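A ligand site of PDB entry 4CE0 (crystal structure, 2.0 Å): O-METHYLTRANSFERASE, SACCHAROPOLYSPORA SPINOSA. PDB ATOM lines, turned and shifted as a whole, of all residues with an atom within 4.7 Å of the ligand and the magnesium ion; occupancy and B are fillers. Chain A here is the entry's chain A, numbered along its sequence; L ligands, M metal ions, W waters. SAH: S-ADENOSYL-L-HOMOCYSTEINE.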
ATOM      1  N   HIS A  52       6.689   4.092  27.041  1.00  0.00           N
ATOM      2  CA  HIS A  52       7.885   3.254  27.039  1.00  0.00           C
ATOM      3  C   HIS A  52       7.605   1.810  27.400  1.00  0.00           C
ATOM      4  O   HIS A  52       8.467   0.934  27.237  1.00  0.00           O
ATOM      5  CB  HIS A  52       8.938   3.842  27.961  1.00  0.00           C
ATOM      6  CG  HIS A  52       9.565   5.089  27.421  1.00  0.00           C
ATOM      7  ND1 HIS A  52      10.004   6.121  28.231  1.00  0.00           N
ATOM      8  CD2 HIS A  52       9.802   5.486  26.151  1.00  0.00           C
ATOM      9  CE1 HIS A  52      10.507   7.081  27.477  1.00  0.00           C
ATOM     10  NE2 HIS A  52      10.385   6.715  26.202  1.00  0.00           N
ATOM     11  N   THR A  53       6.400   1.558  27.871  1.00  0.00           N
ATOM     12  CA  THR A  53       5.909   0.191  28.012  1.00  0.00           C
ATOM     13  C   THR A  53       4.486   0.079  27.536  1.00  0.00           C
ATOM     14  O   THR A  53       3.716   1.030  27.611  1.00  0.00           O
ATOM     15  CB  THR A  53       5.986  -0.316  29.487  1.00  0.00           C
ATOM     16  OG1 THR A  53       5.652  -1.700  29.516  1.00  0.00           O
ATOM     17  CG2 THR A  53       5.010   0.441  30.393  1.00  0.00           C
ATOM     18  N   MET A  54       4.145  -1.126  27.058  1.00  0.00           N
ATOM     19  CA  MET A  54       2.816  -1.440  26.582  1.00  0.00           C
ATOM     20  C   MET A  54       2.039  -2.280  27.607  1.00  0.00           C
ATOM     21  O   MET A  54       0.851  -2.561  27.423  1.00  0.00           O
ATOM     22  CB  MET A  54       2.904  -2.146  25.208  1.00  0.00           C
ATOM     23  CG  MET A  54       3.350  -3.601  25.247  1.00  0.00           C
ATOM     24  SD  MET A  54       3.237  -4.405  23.630  1.00  0.00           S
ATOM     25  CE  MET A  54       4.524  -3.596  22.671  1.00  0.00           C
ATOM     26  N   ILE A  55       2.672  -2.625  28.735  1.00  0.00           N
ATOM     27  CA  ILE A  55       2.020  -3.572  29.651  1.00  0.00           C
ATOM     28  C   ILE A  55       0.928  -3.041  30.563  1.00  0.00           C
ATOM     29  O   ILE A  55       0.232  -3.831  31.181  1.00  0.00           O
ATOM     30  CB  ILE A  55       3.053  -4.407  30.491  1.00  0.00           C
ATOM     31  CG1 ILE A  55       3.669  -3.562  31.586  1.00  0.00           C
ATOM     32  CG2 ILE A  55       4.068  -5.030  29.576  1.00  0.00           C
ATOM     33  CD1 ILE A  55       4.577  -4.327  32.570  1.00  0.00           C
ATOM     34  N   ARG A  59      -0.145  -4.583  35.232  1.00  0.00           N
ATOM     35  CA  ARG A  59       1.021  -5.468  35.125  1.00  0.00           C
ATOM     36  C   ARG A  59       2.312  -4.823  35.701  1.00  0.00           C
ATOM     37  O   ARG A  59       3.199  -5.499  36.189  1.00  0.00           O
ATOM     38  CB  ARG A  59       1.150  -5.980  33.698  1.00  0.00           C
ATOM     39  CG  ARG A  59      -0.141  -6.708  33.245  1.00  0.00           C
ATOM     40  CD  ARG A  59       0.105  -7.858  32.318  1.00  0.00           C
ATOM     41  NE  ARG A  59       0.604  -7.467  31.002  1.00  0.00           N
ATOM     42  CZ  ARG A  59      -0.168  -7.042  30.003  1.00  0.00           C
ATOM     43  NH1 ARG A  59      -1.480  -6.909  30.160  1.00  0.00           N
ATOM     44  NH2 ARG A  59       0.371  -6.764  28.835  1.00  0.00           N
ATOM     45  N   GLU A  81      14.374  -9.336  31.695  1.00  0.00           N
ATOM     46  CA  GLU A  81      13.196  -9.387  30.819  1.00  0.00           C
ATOM     47  C   GLU A  81      13.585  -9.772  29.401  1.00  0.00           C
ATOM     48  O   GLU A  81      14.446  -9.154  28.767  1.00  0.00           O
ATOM     49  CB  GLU A  81      12.366  -8.085  30.814  1.00  0.00           C
ATOM     50  CG  GLU A  81      11.002  -8.263  30.034  1.00  0.00           C
ATOM     51  CD  GLU A  81      10.255  -6.965  29.792  1.00  0.00           C
ATOM     52  OE1 GLU A  81      10.936  -5.953  29.470  1.00  0.00           O
ATOM     53  OE2 GLU A  81       8.995  -6.965  29.911  1.00  0.00           O
ATOM     54  N   GLY A  83      12.221  -9.687  26.066  1.00  0.00           N
ATOM     55  CA  GLY A  83      11.233  -8.947  25.291  1.00  0.00           C
ATOM     56  C   GLY A  83      10.951  -7.617  25.985  1.00  0.00           C
ATOM     57  O   GLY A  83      10.142  -7.553  26.922  1.00  0.00           O
ATOM     58  N   VAL A  84      11.629  -6.560  25.513  1.00  0.00           N
ATOM     59  CA  VAL A  84      11.661  -5.262  26.204  1.00  0.00           C
ATOM     60  C   VAL A  84      11.040  -4.098  25.437  1.00  0.00           C
ATOM     61  O   VAL A  84      10.649  -3.108  26.052  1.00  0.00           O
ATOM     62  CB  VAL A  84      13.112  -4.907  26.630  1.00  0.00           C
ATOM     63  CG1 VAL A  84      13.776  -6.118  27.207  1.00  0.00           C
ATOM     64  CG2 VAL A  84      13.961  -4.300  25.459  1.00  0.00           C
ATOM     65  N   TRP A  85      10.904  -4.239  24.111  1.00  0.00           N
ATOM     66  CA  TRP A  85      10.362  -3.168  23.262  1.00  0.00           C
ATOM     67  C   TRP A  85      11.095  -1.875  23.597  1.00  0.00           C
ATOM     68  O   TRP A  85      12.328  -1.819  23.432  1.00  0.00           O
ATOM     69  CB  TRP A  85       8.857  -3.033  23.444  1.00  0.00           C
ATOM     70  CG  TRP A  85       8.136  -2.174  22.463  1.00  0.00           C
ATOM     71  CD1 TRP A  85       8.280  -2.207  21.105  1.00  0.00           C
ATOM     72  CD2 TRP A  85       7.117  -1.203  22.743  1.00  0.00           C
ATOM     73  NE1 TRP A  85       7.431  -1.284  20.522  1.00  0.00           N
ATOM     74  CE2 TRP A  85       6.713  -0.664  21.496  1.00  0.00           C
ATOM     75  CE3 TRP A  85       6.516  -0.727  23.911  1.00  0.00           C
ATOM     76  CZ2 TRP A  85       5.734   0.340  21.399  1.00  0.00           C
ATOM     77  CZ3 TRP A  85       5.550   0.279  23.811  1.00  0.00           C
ATOM     78  CH2 TRP A  85       5.191   0.807  22.560  1.00  0.00           C
ATOM     79  N   ALA A  89       9.402  -1.675  31.034  1.00  0.00           N
ATOM     80  CA  ALA A  89       9.328  -2.622  32.149  1.00  0.00           C
ATOM     81  C   ALA A  89      10.682  -2.776  32.811  1.00  0.00           C
ATOM     82  O   ALA A  89      10.788  -2.875  34.021  1.00  0.00           O
ATOM     83  CB  ALA A  89       8.807  -3.952  31.682  1.00  0.00           C
ATOM     84  N   ASP A 111      16.837  -8.674  24.328  1.00  0.00           N
ATOM     85  CA  ASP A 111      15.988  -8.478  23.175  1.00  0.00           C
ATOM     86  C   ASP A 111      16.784  -8.642  21.897  1.00  0.00           C
ATOM     87  O   ASP A 111      18.021  -8.628  21.915  1.00  0.00           O
ATOM     88  CB  ASP A 111      15.383  -7.070  23.238  1.00  0.00           C
ATOM     89  CG  ASP A 111      14.129  -6.943  22.384  1.00  0.00           C
ATOM     90  OD1 ASP A 111      14.260  -6.805  21.143  1.00  0.00           O
ATOM     91  OD2 ASP A 111      13.031  -6.954  22.959  1.00  0.00           O
ATOM     92  N   SER A 112      16.087  -8.771  20.770  1.00  0.00           N
ATOM     93  CA  SER A 112      16.767  -8.665  19.467  1.00  0.00           C
ATOM     94  C   SER A 112      17.126  -7.203  19.160  1.00  0.00           C
ATOM     95  O   SER A 112      18.114  -6.944  18.490  1.00  0.00           O
ATOM     96  CB  SER A 112      15.859  -9.162  18.360  1.00  0.00           C
ATOM     97  OG  SER A 112      14.734  -8.309  18.279  1.00  0.00           O
ATOM     98  N   PHE A 113      16.302  -6.272  19.649  1.00  0.00           N
ATOM     99  CA  PHE A 113      16.411  -4.845  19.303  1.00  0.00           C
ATOM    100  C   PHE A 113      16.180  -4.626  17.803  1.00  0.00           C
ATOM    101  O   PHE A 113      16.642  -3.647  17.233  1.00  0.00           O
ATOM    102  CB  PHE A 113      17.733  -4.216  19.793  1.00  0.00           C
ATOM    103  CG  PHE A 113      17.916  -4.281  21.303  1.00  0.00           C
ATOM    104  CD1 PHE A 113      17.238  -3.393  22.143  1.00  0.00           C
ATOM    105  CD2 PHE A 113      18.745  -5.239  21.875  1.00  0.00           C
ATOM    106  CE1 PHE A 113      17.372  -3.478  23.516  1.00  0.00           C
ATOM    107  CE2 PHE A 113      18.891  -5.320  23.266  1.00  0.00           C
ATOM    108  CZ  PHE A 113      18.211  -4.419  24.078  1.00  0.00           C
ATOM    109  N   GLN A 114      15.436  -5.555  17.196  1.00  0.00           N
ATOM    110  CA  GLN A 114      15.010  -5.495  15.799  1.00  0.00           C
ATOM    111  C   GLN A 114      13.562  -5.950  15.662  1.00  0.00           C
ATOM    112  O   GLN A 114      13.072  -6.141  14.558  1.00  0.00           O
ATOM    113  CB  GLN A 114      15.842  -6.419  14.908  1.00  0.00           C
ATOM    114  CG  GLN A 114      17.330  -6.350  15.114  1.00  0.00           C
ATOM    115  CD  GLN A 114      18.024  -7.601  14.619  1.00  0.00           C
ATOM    116  OE1 GLN A 114      17.768  -8.081  13.501  1.00  0.00           O
ATOM    117  NE2 GLN A 114      18.894  -8.165  15.448  1.00  0.00           N
ATOM    118  N   GLY A 115      12.894  -6.193  16.779  1.00  0.00           N
ATOM    119  CA  GLY A 115      11.529  -6.682  16.739  1.00  0.00           C
ATOM    120  C   GLY A 115      11.473  -8.193  16.642  1.00  0.00           C
ATOM    121  O   GLY A 115      12.458  -8.881  16.971  1.00  0.00           O
ATOM    122  N   MET A 116      10.323  -8.687  16.198  1.00  0.00           N
ATOM    123  CA  MET A 116      10.009 -10.115  16.170  1.00  0.00           C
ATOM    124  C   MET A 116      10.721 -10.832  15.022  1.00  0.00           C
ATOM    125  O   MET A 116      10.918 -10.248  13.966  1.00  0.00           O
ATOM    126  CB  MET A 116       8.506 -10.300  15.959  1.00  0.00           C
ATOM    127  CG  MET A 116       7.634  -9.325  16.755  1.00  0.00           C
ATOM    128  SD  MET A 116       7.718  -9.511  18.548  1.00  0.00           S
ATOM    129  CE  MET A 116       7.187 -11.198  18.793  1.00  0.00           C
ATOM    130  N   PRO A 117      11.084 -12.107  15.223  1.00  0.00           N
ATOM    131  CA  PRO A 117      11.623 -12.925  14.119  1.00  0.00           C
ATOM    132  C   PRO A 117      10.533 -13.386  13.124  1.00  0.00           C
ATOM    133  O   PRO A 117       9.352 -13.196  13.411  1.00  0.00           O
ATOM    134  CB  PRO A 117      12.236 -14.125  14.840  1.00  0.00           C
ATOM    135  CG  PRO A 117      11.417 -14.263  16.104  1.00  0.00           C
ATOM    136  CD  PRO A 117      11.005 -12.861  16.490  1.00  0.00           C
ATOM    137  N   LEU A 139       7.490  -2.934  16.392  1.00  0.00           N
ATOM    138  CA  LEU A 139       7.929  -3.539  17.627  1.00  0.00           C
ATOM    139  C   LEU A 139       9.459  -3.579  17.665  1.00  0.00           C
ATOM    140  O   LEU A 139      10.061  -4.049  18.643  1.00  0.00           O
ATOM    141  CB  LEU A 139       7.393  -4.952  17.689  1.00  0.00           C
ATOM    142  CG  LEU A 139       5.866  -4.960  17.747  1.00  0.00           C
ATOM    143  CD1 LEU A 139       5.321  -6.299  17.243  1.00  0.00           C
ATOM    144  CD2 LEU A 139       5.472  -4.699  19.167  1.00  0.00           C
ATOM    145  N   GLY A 165      20.344  -9.793  20.604  1.00  0.00           N
ATOM    146  CA  GLY A 165      20.403 -10.934  19.702  1.00  0.00           C
ATOM    147  C   GLY A 165      19.092 -11.666  19.741  1.00  0.00           C
ATOM    148  O   GLY A 165      18.224 -11.334  20.541  1.00  0.00           O
ATOM    149  N   TRP A 166      18.929 -12.629  18.840  1.00  0.00           N
ATOM    150  CA  TRP A 166      17.800 -13.543  18.920  1.00  0.00           C
ATOM    151  C   TRP A 166      18.030 -14.445  20.112  1.00  0.00           C
ATOM    152  O   TRP A 166      19.140 -14.907  20.328  1.00  0.00           O
ATOM    153  CB  TRP A 166      17.661 -14.321  17.600  1.00  0.00           C
ATOM    154  CG  TRP A 166      17.586 -13.372  16.455  1.00  0.00           C
ATOM    155  CD1 TRP A 166      18.569 -13.086  15.538  1.00  0.00           C
ATOM    156  CD2 TRP A 166      16.469 -12.554  16.113  1.00  0.00           C
ATOM    157  NE1 TRP A 166      18.123 -12.133  14.661  1.00  0.00           N
ATOM    158  CE2 TRP A 166      16.827 -11.797  14.975  1.00  0.00           C
ATOM    159  CE3 TRP A 166      15.191 -12.385  16.657  1.00  0.00           C
ATOM    160  CZ2 TRP A 166      15.954 -10.895  14.375  1.00  0.00           C
ATOM    161  CZ3 TRP A 166      14.325 -11.489  16.053  1.00  0.00           C
ATOM    162  CH2 TRP A 166      14.714 -10.755  14.934  1.00  0.00           C
ATOM    163  N   PHE A 167      16.980 -14.687  20.888  1.00  0.00           N
ATOM    164  CA  PHE A 167      17.086 -15.542  22.083  1.00  0.00           C
ATOM    165  C   PHE A 167      17.789 -16.900  21.809  1.00  0.00           C
ATOM    166  O   PHE A 167      18.609 -17.389  22.603  1.00  0.00           O
ATOM    167  CB  PHE A 167      15.702 -15.811  22.646  1.00  0.00           C
ATOM    168  CG  PHE A 167      14.980 -14.579  23.115  1.00  0.00           C
ATOM    169  CD1 PHE A 167      15.680 -13.415  23.427  1.00  0.00           C
ATOM    170  CD2 PHE A 167      13.603 -14.577  23.215  1.00  0.00           C
ATOM    171  CE1 PHE A 167      14.996 -12.267  23.859  1.00  0.00           C
ATOM    172  CE2 PHE A 167      12.904 -13.443  23.639  1.00  0.00           C
ATOM    173  CZ  PHE A 167      13.610 -12.282  23.970  1.00  0.00           C
ATOM    174  N   ARG A 183      11.100 -12.147  33.666  1.00  0.00           N
ATOM    175  CA  ARG A 183       9.892 -11.649  32.999  1.00  0.00           C
ATOM    176  C   ARG A 183       9.935 -12.005  31.519  1.00  0.00           C
ATOM    177  O   ARG A 183      10.905 -11.707  30.830  1.00  0.00           O
ATOM    178  CB  ARG A 183       9.731 -10.149  33.211  1.00  0.00           C
ATOM    179  CG  ARG A 183       8.387  -9.619  32.738  1.00  0.00           C
ATOM    180  CD  ARG A 183       8.147  -8.127  33.067  1.00  0.00           C
ATOM    181  NE  ARG A 183       6.711  -8.016  33.141  1.00  0.00           N
ATOM    182  CZ  ARG A 183       5.914  -7.867  32.102  1.00  0.00           C
ATOM    183  NH1 ARG A 183       6.394  -7.661  30.875  1.00  0.00           N
ATOM    184  NH2 ARG A 183       4.600  -7.882  32.318  1.00  0.00           N
ATOM    185  N   ASP A 185       8.210 -11.636  27.917  1.00  0.00           N
ATOM    186  CA  ASP A 185       7.296 -10.814  27.156  1.00  0.00           C
ATOM    187  C   ASP A 185       7.706 -10.873  25.704  1.00  0.00           C
ATOM    188  O   ASP A 185       7.772  -9.867  25.024  1.00  0.00           O
ATOM    189  CB  ASP A 185       7.283  -9.374  27.695  1.00  0.00           C
ATOM    190  CG  ASP A 185       5.993  -8.636  27.358  1.00  0.00           C
ATOM    191  OD1 ASP A 185       5.172  -9.171  26.557  1.00  0.00           O
ATOM    192  OD2 ASP A 185       5.781  -7.511  27.911  1.00  0.00           O
ATOM    193  N   GLY A 186       8.055 -12.075  25.266  1.00  0.00           N
ATOM    194  CA  GLY A 186       8.075 -12.409  23.849  1.00  0.00           C
ATOM    195  C   GLY A 186       6.776 -13.154  23.628  1.00  0.00           C
ATOM    196  O   GLY A 186       6.422 -14.054  24.391  1.00  0.00           O
ATOM    197  N   ASP A 187       6.026 -12.774  22.605  1.00  0.00           N
ATOM    198  CA  ASP A 187       4.716 -13.369  22.392  1.00  0.00           C
ATOM    199  C   ASP A 187       4.766 -14.789  21.836  1.00  0.00           C
ATOM    200  O   ASP A 187       3.893 -15.612  22.110  1.00  0.00           O
ATOM    201  CB  ASP A 187       3.934 -12.472  21.447  1.00  0.00           C
ATOM    202  CG  ASP A 187       3.622 -11.122  22.068  1.00  0.00           C
ATOM    203  OD1 ASP A 187       3.061 -11.104  23.188  1.00  0.00           O
ATOM    204  OD2 ASP A 187       3.960 -10.086  21.450  1.00  0.00           O
ATOM    205  N   SER A 191       9.971 -17.930  21.361  1.00  0.00           N
ATOM    206  CA  SER A 191      10.569 -16.919  22.226  1.00  0.00           C
ATOM    207  C   SER A 191      10.376 -17.314  23.684  1.00  0.00           C
ATOM    208  O   SER A 191      11.324 -17.303  24.484  1.00  0.00           O
ATOM    209  CB  SER A 191       9.917 -15.569  21.976  1.00  0.00           C
ATOM    210  OG  SER A 191      10.071 -15.162  20.627  1.00  0.00           O
ATOM    211  N   ASP A 212       3.908 -12.450  30.495  1.00  0.00           N
ATOM    212  CA  ASP A 212       3.133 -11.258  30.264  1.00  0.00           C
ATOM    213  C   ASP A 212       1.855 -11.557  29.470  1.00  0.00           C
ATOM    214  O   ASP A 212       0.872 -10.864  29.637  1.00  0.00           O
ATOM    215  CB  ASP A 212       3.966 -10.173  29.561  1.00  0.00           C
ATOM    216  CG  ASP A 212       3.248  -8.837  29.498  1.00  0.00           C
ATOM    217  OD1 ASP A 212       3.182  -8.167  30.553  1.00  0.00           O
ATOM    218  OD2 ASP A 212       2.723  -8.472  28.426  1.00  0.00           O
ATOM    219  N   ASP A 213       1.908 -12.575  28.602  1.00  0.00           N
ATOM    220  CA  ASP A 213       0.797 -12.922  27.718  1.00  0.00           C
ATOM    221  C   ASP A 213       0.403 -14.380  27.846  1.00  0.00           C
ATOM    222  O   ASP A 213       0.194 -15.082  26.846  1.00  0.00           O
ATOM    223  CB  ASP A 213       1.159 -12.649  26.252  1.00  0.00           C
ATOM    224  CG  ASP A 213       1.312 -11.188  25.974  1.00  0.00           C
ATOM    225  OD1 ASP A 213       0.282 -10.524  25.716  1.00  0.00           O
ATOM    226  OD2 ASP A 213       2.461 -10.691  26.037  1.00  0.00           O
HETATM  227  N   SAH L   1       6.366  -3.013  26.403  1.00  0.00           N
HETATM  228  CA  SAH L   1       6.597  -4.468  26.358  1.00  0.00           C
HETATM  229  CB  SAH L   1       7.395  -4.985  25.187  1.00  0.00           C
HETATM  230  CG  SAH L   1       7.569  -6.443  24.767  1.00  0.00           C
HETATM  231  SD  SAH L   1       7.180  -6.436  22.991  1.00  0.00           S
HETATM  232  C   SAH L   1       7.392  -4.590  27.592  1.00  0.00           C
HETATM  233  O   SAH L   1       8.013  -5.628  27.715  1.00  0.00           O
HETATM  234  OXT SAH L   1       7.209  -3.436  28.343  1.00  0.00           O
HETATM  235  C5' SAH L   1       8.034  -7.947  22.414  1.00  0.00           C
HETATM  236  C4' SAH L   1       9.558  -7.821  22.345  1.00  0.00           C
HETATM  237  O4' SAH L   1      10.153  -9.108  22.253  1.00  0.00           O
HETATM  238  C3' SAH L   1      10.086  -7.063  21.126  1.00  0.00           C
HETATM  239  O3' SAH L   1      10.874  -5.997  21.606  1.00  0.00           O
HETATM  240  C2' SAH L   1      10.895  -8.056  20.282  1.00  0.00           C
HETATM  241  O2' SAH L   1      12.045  -7.557  19.563  1.00  0.00           O
HETATM  242  C1' SAH L   1      11.238  -9.109  21.330  1.00  0.00           C
HETATM  243  N9  SAH L   1      11.415 -10.497  20.847  1.00  0.00           N
HETATM  244  C8  SAH L   1      10.400 -11.393  20.590  1.00  0.00           C
HETATM  245  N7  SAH L   1      10.954 -12.561  20.245  1.00  0.00           N
HETATM  246  C5  SAH L   1      12.300 -12.452  20.300  1.00  0.00           C
HETATM  247  C6  SAH L   1      13.358 -13.324  20.048  1.00  0.00           C
HETATM  248  N6  SAH L   1      13.132 -14.589  19.663  1.00  0.00           N
HETATM  249  N1  SAH L   1      14.654 -12.902  20.182  1.00  0.00           N
HETATM  250  C2  SAH L   1      14.944 -11.609  20.595  1.00  0.00           C
HETATM  251  N3  SAH L   1      13.899 -10.750  20.810  1.00  0.00           N
HETATM  252  C4  SAH L   1      12.596 -11.165  20.710  1.00  0.00           C
HETATM  253 MG    MG M   1       3.166  -8.791  26.507  1.00  0.00          MG
HETATM  254  O   HOH W   1       3.322  -8.712  24.434  1.00  0.00           O
HETATM  255  O   HOH W   2       1.113  -8.013  25.884  1.00  0.00           O
HETATM  256  O   HOH W   3      10.557  -3.269  28.863  1.00  0.00           O
HETATM  257  O   HOH W   4      12.707  -4.519  19.259  1.00  0.00           O
HETATM  258  O   HOH W   5      14.943 -16.980  19.053  1.00  0.00           O
HETATM  259  O   HOH W   6       3.445  -6.664  26.201  1.00  0.00           O
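The side-chain carboxylate of Asp 185 sits close to an oxygen (O) of the ligand.
OG1 of Thr 53 sits at hydrogen-bond distance from OXT of the ligand.
OD2 of Asp 111 lies within hydrogen-bond range of O3' of the ligand, at 2.7 Å.
An oxygen (O) of the ligand lies close to the side-chain carboxylate (OE2) of Glu 81.
The side-chain hydroxyl (OG) of Ser 191 sits at hydrogen-bond distance from a nitrogen (N7) of the ligand.
The backbone NH of Gly 115 sits close to an oxygen (O2') of the ligand, 3.2 Å away.
An oxygen (O2') of the ligand lies within hydrogen-bond range of the backbone carbonyl oxygen (O) of Gly 115.
N of Ser 112 is in hydrogen-bond range of N3 of the ligand (3.0 Å).
OG of Ser 112 is in hydrogen-bond range of O2' of the ligand (3.1 Å).
An oxygen (O) of the ligand sits close to the backbone carbonyl oxygen (O) of Gly 83 (3.0 Å).
A nitrogen (N) of the ligand lies close to the backbone NH (N) of Met 54 (3.0 Å).
An oxygen (O3') of the ligand lies within hydrogen-bond range of the backbone NH (N) of Trp 85.
N of Phe 167 sits at hydrogen-bond distance from N1 of the ligand, at 3.0 Å.
The guanidinium group (NE) of Arg 59 lies within salt-bridge range of the side-chain carboxylate (OD1) of Asp 212.
The side-chain carboxylate of Asp 185 is in salt-bridge range of the guanidinium group of Arg 183 (3.0 Å).
O of Asp 111 is in hydrogen-bond range of N of Gly 165 (2.9 Å).
The side-chain carboxylate (OD2) of Asp 111 lies within hydrogen-bond range of the backbone NH (N) of Val 84 (2.9 Å).
The side-chain carboxylate (OD1) of Asp 111 lies within hydrogen-bond range of the backbone NH (N) of Phe 113.
OE2 of Glu 81 lies within salt-bridge range of NH1 of Arg 183.
O of Gly 115 sits at hydrogen-bond distance from OG of Ser 112 (2.7 Å).
N of Ser 112 lies close to O of Gly 165 (3.3 Å).
Ile 55 touches the ligand (CG2 to OXT, 3.7 Å).
C of Val 84 touches CB of the ligand, 3.8 Å away.
CB of Ala 89 touches OXT of the ligand, at 3.7 Å.
CE of Met 116 touches C8 of the ligand, at 3.7 Å.
CD of Pro 117 touches N7 of the ligand, at 3.8 Å.
Leu 139 touches the ligand.
Gly 165 touches the ligand (O to C2, 3.3 Å).
Trp 166 touches the ligand (CA to N1, 3.4 Å).
Within 4 Å of the ligand: Thr 53, Met 54, Ile 55, Glu 81, Gly 83, Val 84, Trp 85, Ala 89, Asp 111, Ser 112, Gly 115, Met 116, Pro 117, Leu 139, Gly 165, Trp 166, Phe 167, Asp 185 and Ser 191.
Three residues have an atom within 4 Å of the magnesium ion: Asp 185, Asp 212 and Asp 213.
The nearest printed residue that does not touch the magnesium ion is Asp 187 (4.05 Å).
The magnesium ion is bound by the side-chain carboxylate (OD2) of Asp 212 (2.0 Å).
The side-chain carboxylate (OD1) of Asp 185 binds the magnesium ion, at 2.0 Å.
The magnesium ion is bound by water W1.
The magnesium ion is bound by OD2 of Asp 213 (2.1 Å).
Water W6 binds the magnesium ion, 2.2 Å away.
Water W2 is bound to the magnesium ion (2.3 Å).
The magnesium ion has six donor atoms within binding distance.
Water W6 bridges the side-chain carboxylate of Asp 185 (3.0 Å) and the side-chain sulfur of Met 54 (3.4 Å).
Water W2 lies within hydrogen-bond range of the side-chain carboxylate of Asp 213 (2.7 Å) and the guanidinium group of Arg 59 (3.3 Å).
Water W4 lies within hydrogen-bond range of the backbone carbonyl oxygen (O) of Leu 139, the backbone NH (N) of Gly 115, an oxygen (O2') of the ligand and the side-chain carboxylate (OD1) of Asp 111.
Water W3 lies within hydrogen-bond range of OE1 of Glu 81 (2.8 Å), O of Val 84 (2.8 Å), N of Ala 89 (2.9 Å) and OXT of the ligand (3.4 Å).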
